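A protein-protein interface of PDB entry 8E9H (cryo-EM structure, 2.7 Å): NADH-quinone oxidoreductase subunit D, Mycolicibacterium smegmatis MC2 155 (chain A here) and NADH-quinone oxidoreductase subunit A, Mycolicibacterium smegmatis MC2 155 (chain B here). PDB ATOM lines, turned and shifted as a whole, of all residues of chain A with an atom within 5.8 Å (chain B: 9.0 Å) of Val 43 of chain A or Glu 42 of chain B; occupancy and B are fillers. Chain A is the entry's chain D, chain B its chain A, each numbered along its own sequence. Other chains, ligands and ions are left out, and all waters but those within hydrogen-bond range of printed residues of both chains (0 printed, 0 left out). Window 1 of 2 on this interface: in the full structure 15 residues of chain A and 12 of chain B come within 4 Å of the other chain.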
ATOM      1  N   ILE A  41       7.199  18.183 -13.850  1.00  0.00           N
ATOM      2  CA  ILE A  41       8.641  18.248 -14.024  1.00  0.00           C
ATOM      3  C   ILE A  41       8.972  18.012 -15.490  1.00  0.00           C
ATOM      4  O   ILE A  41       8.209  17.399 -16.234  1.00  0.00           O
ATOM      5  CB  ILE A  41       9.362  17.228 -13.128  1.00  0.00           C
ATOM      6  CG1 ILE A  41       9.142  17.542 -11.653  1.00  0.00           C
ATOM      7  CG2 ILE A  41      10.851  17.226 -13.429  1.00  0.00           C
ATOM      8  CD1 ILE A  41       9.526  16.402 -10.738  1.00  0.00           C
ATOM      9  N   VAL A  42      10.121  18.519 -15.917  1.00  0.00           N
ATOM     10  CA  VAL A  42      10.690  18.170 -17.210  1.00  0.00           C
ATOM     11  C   VAL A  42      12.093  17.643 -16.960  1.00  0.00           C
ATOM     12  O   VAL A  42      12.935  18.347 -16.395  1.00  0.00           O
ATOM     13  CB  VAL A  42      10.702  19.363 -18.181  1.00  0.00           C
ATOM     14  CG1 VAL A  42      11.484  20.518 -17.605  1.00  0.00           C
ATOM     15  CG2 VAL A  42      11.278  18.944 -19.514  1.00  0.00           C
ATOM     16  N   VAL A  43      12.335  16.403 -17.363  1.00  0.00           N
ATOM     17  CA  VAL A  43      13.558  15.695 -17.013  1.00  0.00           C
ATOM     18  C   VAL A  43      14.179  15.139 -18.281  1.00  0.00           C
ATOM     19  O   VAL A  43      13.480  14.618 -19.155  1.00  0.00           O
ATOM     20  CB  VAL A  43      13.281  14.564 -16.003  1.00  0.00           C
ATOM     21  CG1 VAL A  43      12.386  13.510 -16.619  1.00  0.00           C
ATOM     22  CG2 VAL A  43      14.579  13.950 -15.518  1.00  0.00           C
ATOM     23  N   ASN A  44      15.497  15.248 -18.379  1.00  0.00           N
ATOM     24  CA  ASN A  44      16.232  14.643 -19.479  1.00  0.00           C
ATOM     25  C   ASN A  44      16.464  13.178 -19.157  1.00  0.00           C
ATOM     26  O   ASN A  44      17.303  12.848 -18.316  1.00  0.00           O
ATOM     27  CB  ASN A  44      17.561  15.356 -19.694  1.00  0.00           C
ATOM     28  CG  ASN A  44      17.389  16.817 -20.006  1.00  0.00           C
ATOM     29  OD1 ASN A  44      17.307  17.207 -21.168  1.00  0.00           O
ATOM     30  ND2 ASN A  44      17.328  17.637 -18.969  1.00  0.00           N
ATOM     31  N   MET A  45      15.725  12.289 -19.821  1.00  0.00           N
ATOM     32  CA  MET A  45      16.127  10.891 -19.809  1.00  0.00           C
ATOM     33  C   MET A  45      17.539  10.785 -20.359  1.00  0.00           C
ATOM     34  O   MET A  45      18.266   9.829 -20.075  1.00  0.00           O
ATOM     35  CB  MET A  45      15.153  10.053 -20.628  1.00  0.00           C
ATOM     36  CG  MET A  45      15.409   8.565 -20.576  1.00  0.00           C
ATOM     37  SD  MET A  45      15.199   7.874 -18.931  1.00  0.00           S
ATOM     38  CE  MET A  45      13.420   7.935 -18.767  1.00  0.00           C
ATOM     39  N   GLY A  46      17.926  11.758 -21.178  1.00  0.00           N
ATOM     40  CA  GLY A  46      19.304  12.132 -21.359  1.00  0.00           C
ATOM     41  C   GLY A  46      20.131  11.111 -22.098  1.00  0.00           C
ATOM     42  O   GLY A  46      19.794   9.927 -22.158  1.00  0.00           O
ATOM     43  N   PRO A  47      21.241  11.555 -22.678  1.00  0.00           N
ATOM     44  CA  PRO A  47      22.126  10.610 -23.360  1.00  0.00           C
ATOM     45  C   PRO A  47      22.686   9.582 -22.398  1.00  0.00           C
ATOM     46  O   PRO A  47      22.551   8.377 -22.620  1.00  0.00           O
ATOM     47  CB  PRO A  47      23.225  11.509 -23.939  1.00  0.00           C
ATOM     48  CG  PRO A  47      22.640  12.865 -23.963  1.00  0.00           C
ATOM     49  CD  PRO A  47      21.730  12.937 -22.795  1.00  0.00           C
ATOM     50  N   LEU A  58      15.917  11.424 -24.409  1.00  0.00           N
ATOM     51  CA  LEU A  58      14.481  11.572 -24.230  1.00  0.00           C
ATOM     52  C   LEU A  58      14.197  12.659 -23.203  1.00  0.00           C
ATOM     53  O   LEU A  58      14.503  12.504 -22.019  1.00  0.00           O
ATOM     54  CB  LEU A  58      13.857  10.249 -23.799  1.00  0.00           C
ATOM     55  CG  LEU A  58      13.269   9.401 -24.919  1.00  0.00           C
ATOM     56  CD1 LEU A  58      14.364   8.804 -25.765  1.00  0.00           C
ATOM     57  CD2 LEU A  58      12.405   8.311 -24.331  1.00  0.00           C
ATOM     58  N   ILE A  59      13.628  13.770 -23.660  1.00  0.00           N
ATOM     59  CA  ILE A  59      13.195  14.856 -22.791  1.00  0.00           C
ATOM     60  C   ILE A  59      11.733  14.608 -22.466  1.00  0.00           C
ATOM     61  O   ILE A  59      10.871  14.714 -23.345  1.00  0.00           O
ATOM     62  CB  ILE A  59      13.383  16.230 -23.449  1.00  0.00           C
ATOM     63  CG1 ILE A  59      14.831  16.413 -23.897  1.00  0.00           C
ATOM     64  CG2 ILE A  59      12.985  17.334 -22.492  1.00  0.00           C
ATOM     65  CD1 ILE A  59      15.050  16.110 -25.352  1.00  0.00           C
ATOM     66  N   LEU A  60      11.452  14.272 -21.211  1.00  0.00           N
ATOM     67  CA  LEU A  60      10.124  13.844 -20.800  1.00  0.00           C
ATOM     68  C   LEU A  60       9.543  14.865 -19.838  1.00  0.00           C
ATOM     69  O   LEU A  60      10.151  15.172 -18.809  1.00  0.00           O
ATOM     70  CB  LEU A  60      10.183  12.466 -20.142  1.00  0.00           C
ATOM     71  CG  LEU A  60      10.828  11.371 -20.987  1.00  0.00           C
ATOM     72  CD1 LEU A  60      10.822  10.061 -20.236  1.00  0.00           C
ATOM     73  CD2 LEU A  60      10.115  11.225 -22.314  1.00  0.00           C
ATOM     74  N   GLU A  61       8.375  15.392 -20.180  1.00  0.00           N
ATOM     75  CA  GLU A  61       7.584  16.162 -19.238  1.00  0.00           C
ATOM     76  C   GLU A  61       6.635  15.216 -18.523  1.00  0.00           C
ATOM     77  O   GLU A  61       5.789  14.579 -19.161  1.00  0.00           O
ATOM     78  CB  GLU A  61       6.802  17.253 -19.963  1.00  0.00           C
ATOM     79  CG  GLU A  61       5.997  18.148 -19.047  1.00  0.00           C
ATOM     80  CD  GLU A  61       5.098  19.090 -19.814  1.00  0.00           C
ATOM     81  OE1 GLU A  61       5.536  19.614 -20.859  1.00  0.00           O
ATOM     82  OE2 GLU A  61       3.949  19.302 -19.376  1.00  0.00           O
ATOM     83  N   ILE A  62       6.776  15.129 -17.204  1.00  0.00           N
ATOM     84  CA  ILE A  62       6.090  14.138 -16.387  1.00  0.00           C
ATOM     85  C   ILE A  62       5.279  14.849 -15.315  1.00  0.00           C
ATOM     86  O   ILE A  62       5.791  15.737 -14.622  1.00  0.00           O
ATOM     87  CB  ILE A  62       7.087  13.152 -15.751  1.00  0.00           C
ATOM     88  CG1 ILE A  62       7.920  13.848 -14.675  1.00  0.00           C
ATOM     89  CG2 ILE A  62       7.997  12.573 -16.807  1.00  0.00           C
ATOM     90  CD1 ILE A  62       9.045  13.001 -14.147  1.00  0.00           C
ATOM     91  N   SER B  36      30.725  21.944 -12.122  1.00  0.00           N
ATOM     92  CA  SER B  36      30.018  20.889 -12.837  1.00  0.00           C
ATOM     93  C   SER B  36      29.851  19.650 -11.973  1.00  0.00           C
ATOM     94  O   SER B  36      28.814  18.983 -12.043  1.00  0.00           O
ATOM     95  CB  SER B  36      30.756  20.540 -14.125  1.00  0.00           C
ATOM     96  OG  SER B  36      30.901  21.683 -14.947  1.00  0.00           O
ATOM     97  N   GLU B  39      26.904  20.378  -9.291  1.00  0.00           N
ATOM     98  CA  GLU B  39      25.537  20.601  -9.730  1.00  0.00           C
ATOM     99  C   GLU B  39      24.825  19.272  -9.961  1.00  0.00           C
ATOM    100  O   GLU B  39      25.445  18.214 -10.090  1.00  0.00           O
ATOM    101  CB  GLU B  39      25.509  21.452 -10.996  1.00  0.00           C
ATOM    102  CG  GLU B  39      26.061  20.774 -12.224  1.00  0.00           C
ATOM    103  CD  GLU B  39      26.260  21.744 -13.370  1.00  0.00           C
ATOM    104  OE1 GLU B  39      26.129  22.964 -13.145  1.00  0.00           O
ATOM    105  OE2 GLU B  39      26.548  21.289 -14.495  1.00  0.00           O
ATOM    106  N   ALA B  40      23.498  19.342 -10.007  1.00  0.00           N
ATOM    107  CA  ALA B  40      22.680  18.142 -10.042  1.00  0.00           C
ATOM    108  C   ALA B  40      23.030  17.279 -11.245  1.00  0.00           C
ATOM    109  O   ALA B  40      23.532  17.755 -12.265  1.00  0.00           O
ATOM    110  CB  ALA B  40      21.199  18.511 -10.087  1.00  0.00           C
ATOM    111  N   TYR B  41      22.750  15.986 -11.116  1.00  0.00           N
ATOM    112  CA  TYR B  41      22.942  15.030 -12.196  1.00  0.00           C
ATOM    113  C   TYR B  41      21.670  14.980 -13.027  1.00  0.00           C
ATOM    114  O   TYR B  41      20.589  14.710 -12.496  1.00  0.00           O
ATOM    115  CB  TYR B  41      23.271  13.641 -11.659  1.00  0.00           C
ATOM    116  CG  TYR B  41      23.114  12.561 -12.694  1.00  0.00           C
ATOM    117  CD1 TYR B  41      24.078  12.364 -13.668  1.00  0.00           C
ATOM    118  CD2 TYR B  41      21.993  11.752 -12.711  1.00  0.00           C
ATOM    119  CE1 TYR B  41      23.936  11.386 -14.616  1.00  0.00           C
ATOM    120  CE2 TYR B  41      21.843  10.773 -13.658  1.00  0.00           C
ATOM    121  CZ  TYR B  41      22.818  10.591 -14.607  1.00  0.00           C
ATOM    122  OH  TYR B  41      22.674   9.612 -15.557  1.00  0.00           O
ATOM    123  N   GLU B  42      21.802  15.236 -14.325  1.00  0.00           N
ATOM    124  CA  GLU B  42      20.670  15.245 -15.243  1.00  0.00           C
ATOM    125  C   GLU B  42      21.046  14.470 -16.504  1.00  0.00           C
ATOM    126  O   GLU B  42      20.812  14.900 -17.630  1.00  0.00           O
ATOM    127  CB  GLU B  42      20.258  16.679 -15.560  1.00  0.00           C
ATOM    128  CG  GLU B  42      18.950  16.805 -16.313  1.00  0.00           C
ATOM    129  CD  GLU B  42      17.778  16.220 -15.553  1.00  0.00           C
ATOM    130  OE1 GLU B  42      17.863  16.123 -14.313  1.00  0.00           O
ATOM    131  OE2 GLU B  42      16.771  15.862 -16.197  1.00  0.00           O
ATOM    132  N   CYS B  43      21.652  13.303 -16.300  1.00  0.00           N
ATOM    133  CA  CYS B  43      22.056  12.430 -17.398  1.00  0.00           C
ATOM    134  C   CYS B  43      23.029  13.130 -18.340  1.00  0.00           C
ATOM    135  O   CYS B  43      23.074  12.833 -19.533  1.00  0.00           O
ATOM    136  CB  CYS B  43      20.837  11.921 -18.167  1.00  0.00           C
ATOM    137  SG  CYS B  43      19.773  10.826 -17.214  1.00  0.00           S
ATOM    138  N   GLY B  44      23.814  14.060 -17.807  1.00  0.00           N
ATOM    139  CA  GLY B  44      24.848  14.713 -18.582  1.00  0.00           C
ATOM    140  C   GLY B  44      24.442  16.064 -19.125  1.00  0.00           C
ATOM    141  O   GLY B  44      25.297  16.898 -19.428  1.00  0.00           O
ATOM    142  N   ILE B  45      23.136  16.298 -19.257  1.00  0.00           N
ATOM    143  CA  ILE B  45      22.679  17.590 -19.735  1.00  0.00           C
ATOM    144  C   ILE B  45      22.861  18.636 -18.639  1.00  0.00           C
ATOM    145  O   ILE B  45      22.901  18.328 -17.443  1.00  0.00           O
ATOM    146  CB  ILE B  45      21.214  17.515 -20.188  1.00  0.00           C
ATOM    147  CG1 ILE B  45      21.044  16.451 -21.273  1.00  0.00           C
ATOM    148  CG2 ILE B  45      20.742  18.857 -20.700  1.00  0.00           C
ATOM    149  CD1 ILE B  45      22.008  16.579 -22.425  1.00  0.00           C
ATOM    150  N   ASP B  46      22.978  19.889 -19.060  1.00  0.00           N
ATOM    151  CA  ASP B  46      23.091  20.971 -18.098  1.00  0.00           C
ATOM    152  C   ASP B  46      21.825  21.039 -17.249  1.00  0.00           C
ATOM    153  O   ASP B  46      20.715  20.983 -17.784  1.00  0.00           O
ATOM    154  CB  ASP B  46      23.307  22.306 -18.805  1.00  0.00           C
ATOM    155  CG  ASP B  46      24.590  22.344 -19.603  1.00  0.00           C
ATOM    156  OD1 ASP B  46      25.332  21.340 -19.588  1.00  0.00           O
ATOM    157  OD2 ASP B  46      24.859  23.380 -20.245  1.00  0.00           O
ATOM    158  N   PRO B  47      21.953  21.161 -15.929  1.00  0.00           N
ATOM    159  CA  PRO B  47      20.755  21.235 -15.091  1.00  0.00           C
ATOM    160  C   PRO B  47      19.921  22.454 -15.444  1.00  0.00           C
ATOM    161  O   PRO B  47      20.450  23.504 -15.810  1.00  0.00           O
ATOM    162  CB  PRO B  47      21.322  21.325 -13.672  1.00  0.00           C
ATOM    163  CG  PRO B  47      22.668  21.909 -13.852  1.00  0.00           C
ATOM    164  CD  PRO B  47      23.179  21.336 -15.135  1.00  0.00           C
ATOM    165  N   LEU B  48      18.611  22.304 -15.335  1.00  0.00           N
ATOM    166  CA  LEU B  48      17.716  23.409 -15.636  1.00  0.00           C
ATOM    167  C   LEU B  48      18.073  24.592 -14.742  1.00  0.00           C
ATOM    168  O   LEU B  48      18.370  24.392 -13.557  1.00  0.00           O
ATOM    169  CB  LEU B  48      16.266  22.984 -15.417  1.00  0.00           C
ATOM    170  CG  LEU B  48      15.166  23.936 -15.874  1.00  0.00           C
ATOM    171  CD1 LEU B  48      15.148  24.068 -17.381  1.00  0.00           C
ATOM    172  CD2 LEU B  48      13.825  23.438 -15.377  1.00  0.00           C
ATOM    173  N   THR B  56       8.682  24.909 -12.100  1.00  0.00           N
ATOM    174  CA  THR B  56       8.368  23.528 -12.427  1.00  0.00           C
ATOM    175  C   THR B  56       8.811  22.616 -11.293  1.00  0.00           C
ATOM    176  O   THR B  56       9.758  22.921 -10.562  1.00  0.00           O
ATOM    177  CB  THR B  56       9.054  23.087 -13.726  1.00  0.00           C
ATOM    178  OG1 THR B  56      10.456  22.907 -13.492  1.00  0.00           O
ATOM    179  CG2 THR B  56       8.853  24.126 -14.817  1.00  0.00           C
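OH of Tyr 41 of chain B lies close to SG of Cys 43 of chain B (3.6 Å). The backbone NH (N) of Val 43 of chain A is in hydrogen-bond range of the backbone carbonyl oxygen (O) of Leu 60 of chain A, at 2.9 Å. The backbone NH (N) of Met 45 of chain A is in hydrogen-bond range of the backbone carbonyl oxygen (O) of Leu 58 of chain A, 2.5 Å away.
Val 43 of chain A touches Glu 42 of chain B (CG2 to OE2, 3.0 Å). Ile 45 of chain B touches Asn 44 of chain A. Gly 46 of chain A touches Cys 43 of chain B. Cys 43 of chain B touches Pro 47 of chain A (O to CD, 3.5 Å). Pro 47 of chain A touches Ile 45 of chain B.
Of the 12 printed residues of chain A, 5 touch a printed residue of chain B. Of the 12 printed residues of chain B, 3 touch a printed residue of chain A. Hydrophobic or aromatic side chains of chain B within 4 Å of the printed part of chain A: Ile 45. Among the printed residues, 8 pairs touch across the chains. Among the printed residues, no Asp or Glu carboxylate lies within 4 Å of a Lys or Arg side-chain nitrogen of the other chain.
The side-chain sulfur (SG) of Cys 43 of chain B sits at hydrogen-bond distance from the backbone carbonyl oxygen (O) of Met 45 of chain A (3.4 Å). The side-chain carboxylate (OE2) of Glu 42 of chain B is in hydrogen-bond range of the backbone NH (N) of Asn 44 of chain A, at 2.6 Å. O of Asn 44 of chain A is in hydrogen-bond range of SG of Cys 43 of chain B (3.4 Å).
Val 43 of chain A touches one residue of chain B. Of chain A, only Val 43 and Asn 44 come within 4 Å of Glu 42 of chain B. No residue of chain B comes within 4 Å of Val 42 of chain A. Of chain B, only Glu 42 (2.6 Å), Cys 43 (3.4 Å) and Ile 45 (3.8 Å) come within 4 Å of Asn 44 of chain A. Printed residues of chain B within 4 Å of Pro 47 of chain A: Cys 43 (3.5 Å) and Ile 45 (3.7 Å). Printed residues of chain B within 4 Å of Met 45 of chain A: Cys 43. The nearest residue of chain B that does not touch Val 43 of chain A is Cys 43 of chain B (6.3 Å). The nearest residue of chain A that does not touch Glu 42 of chain B is Val 42 of chain A (4.6 Å).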
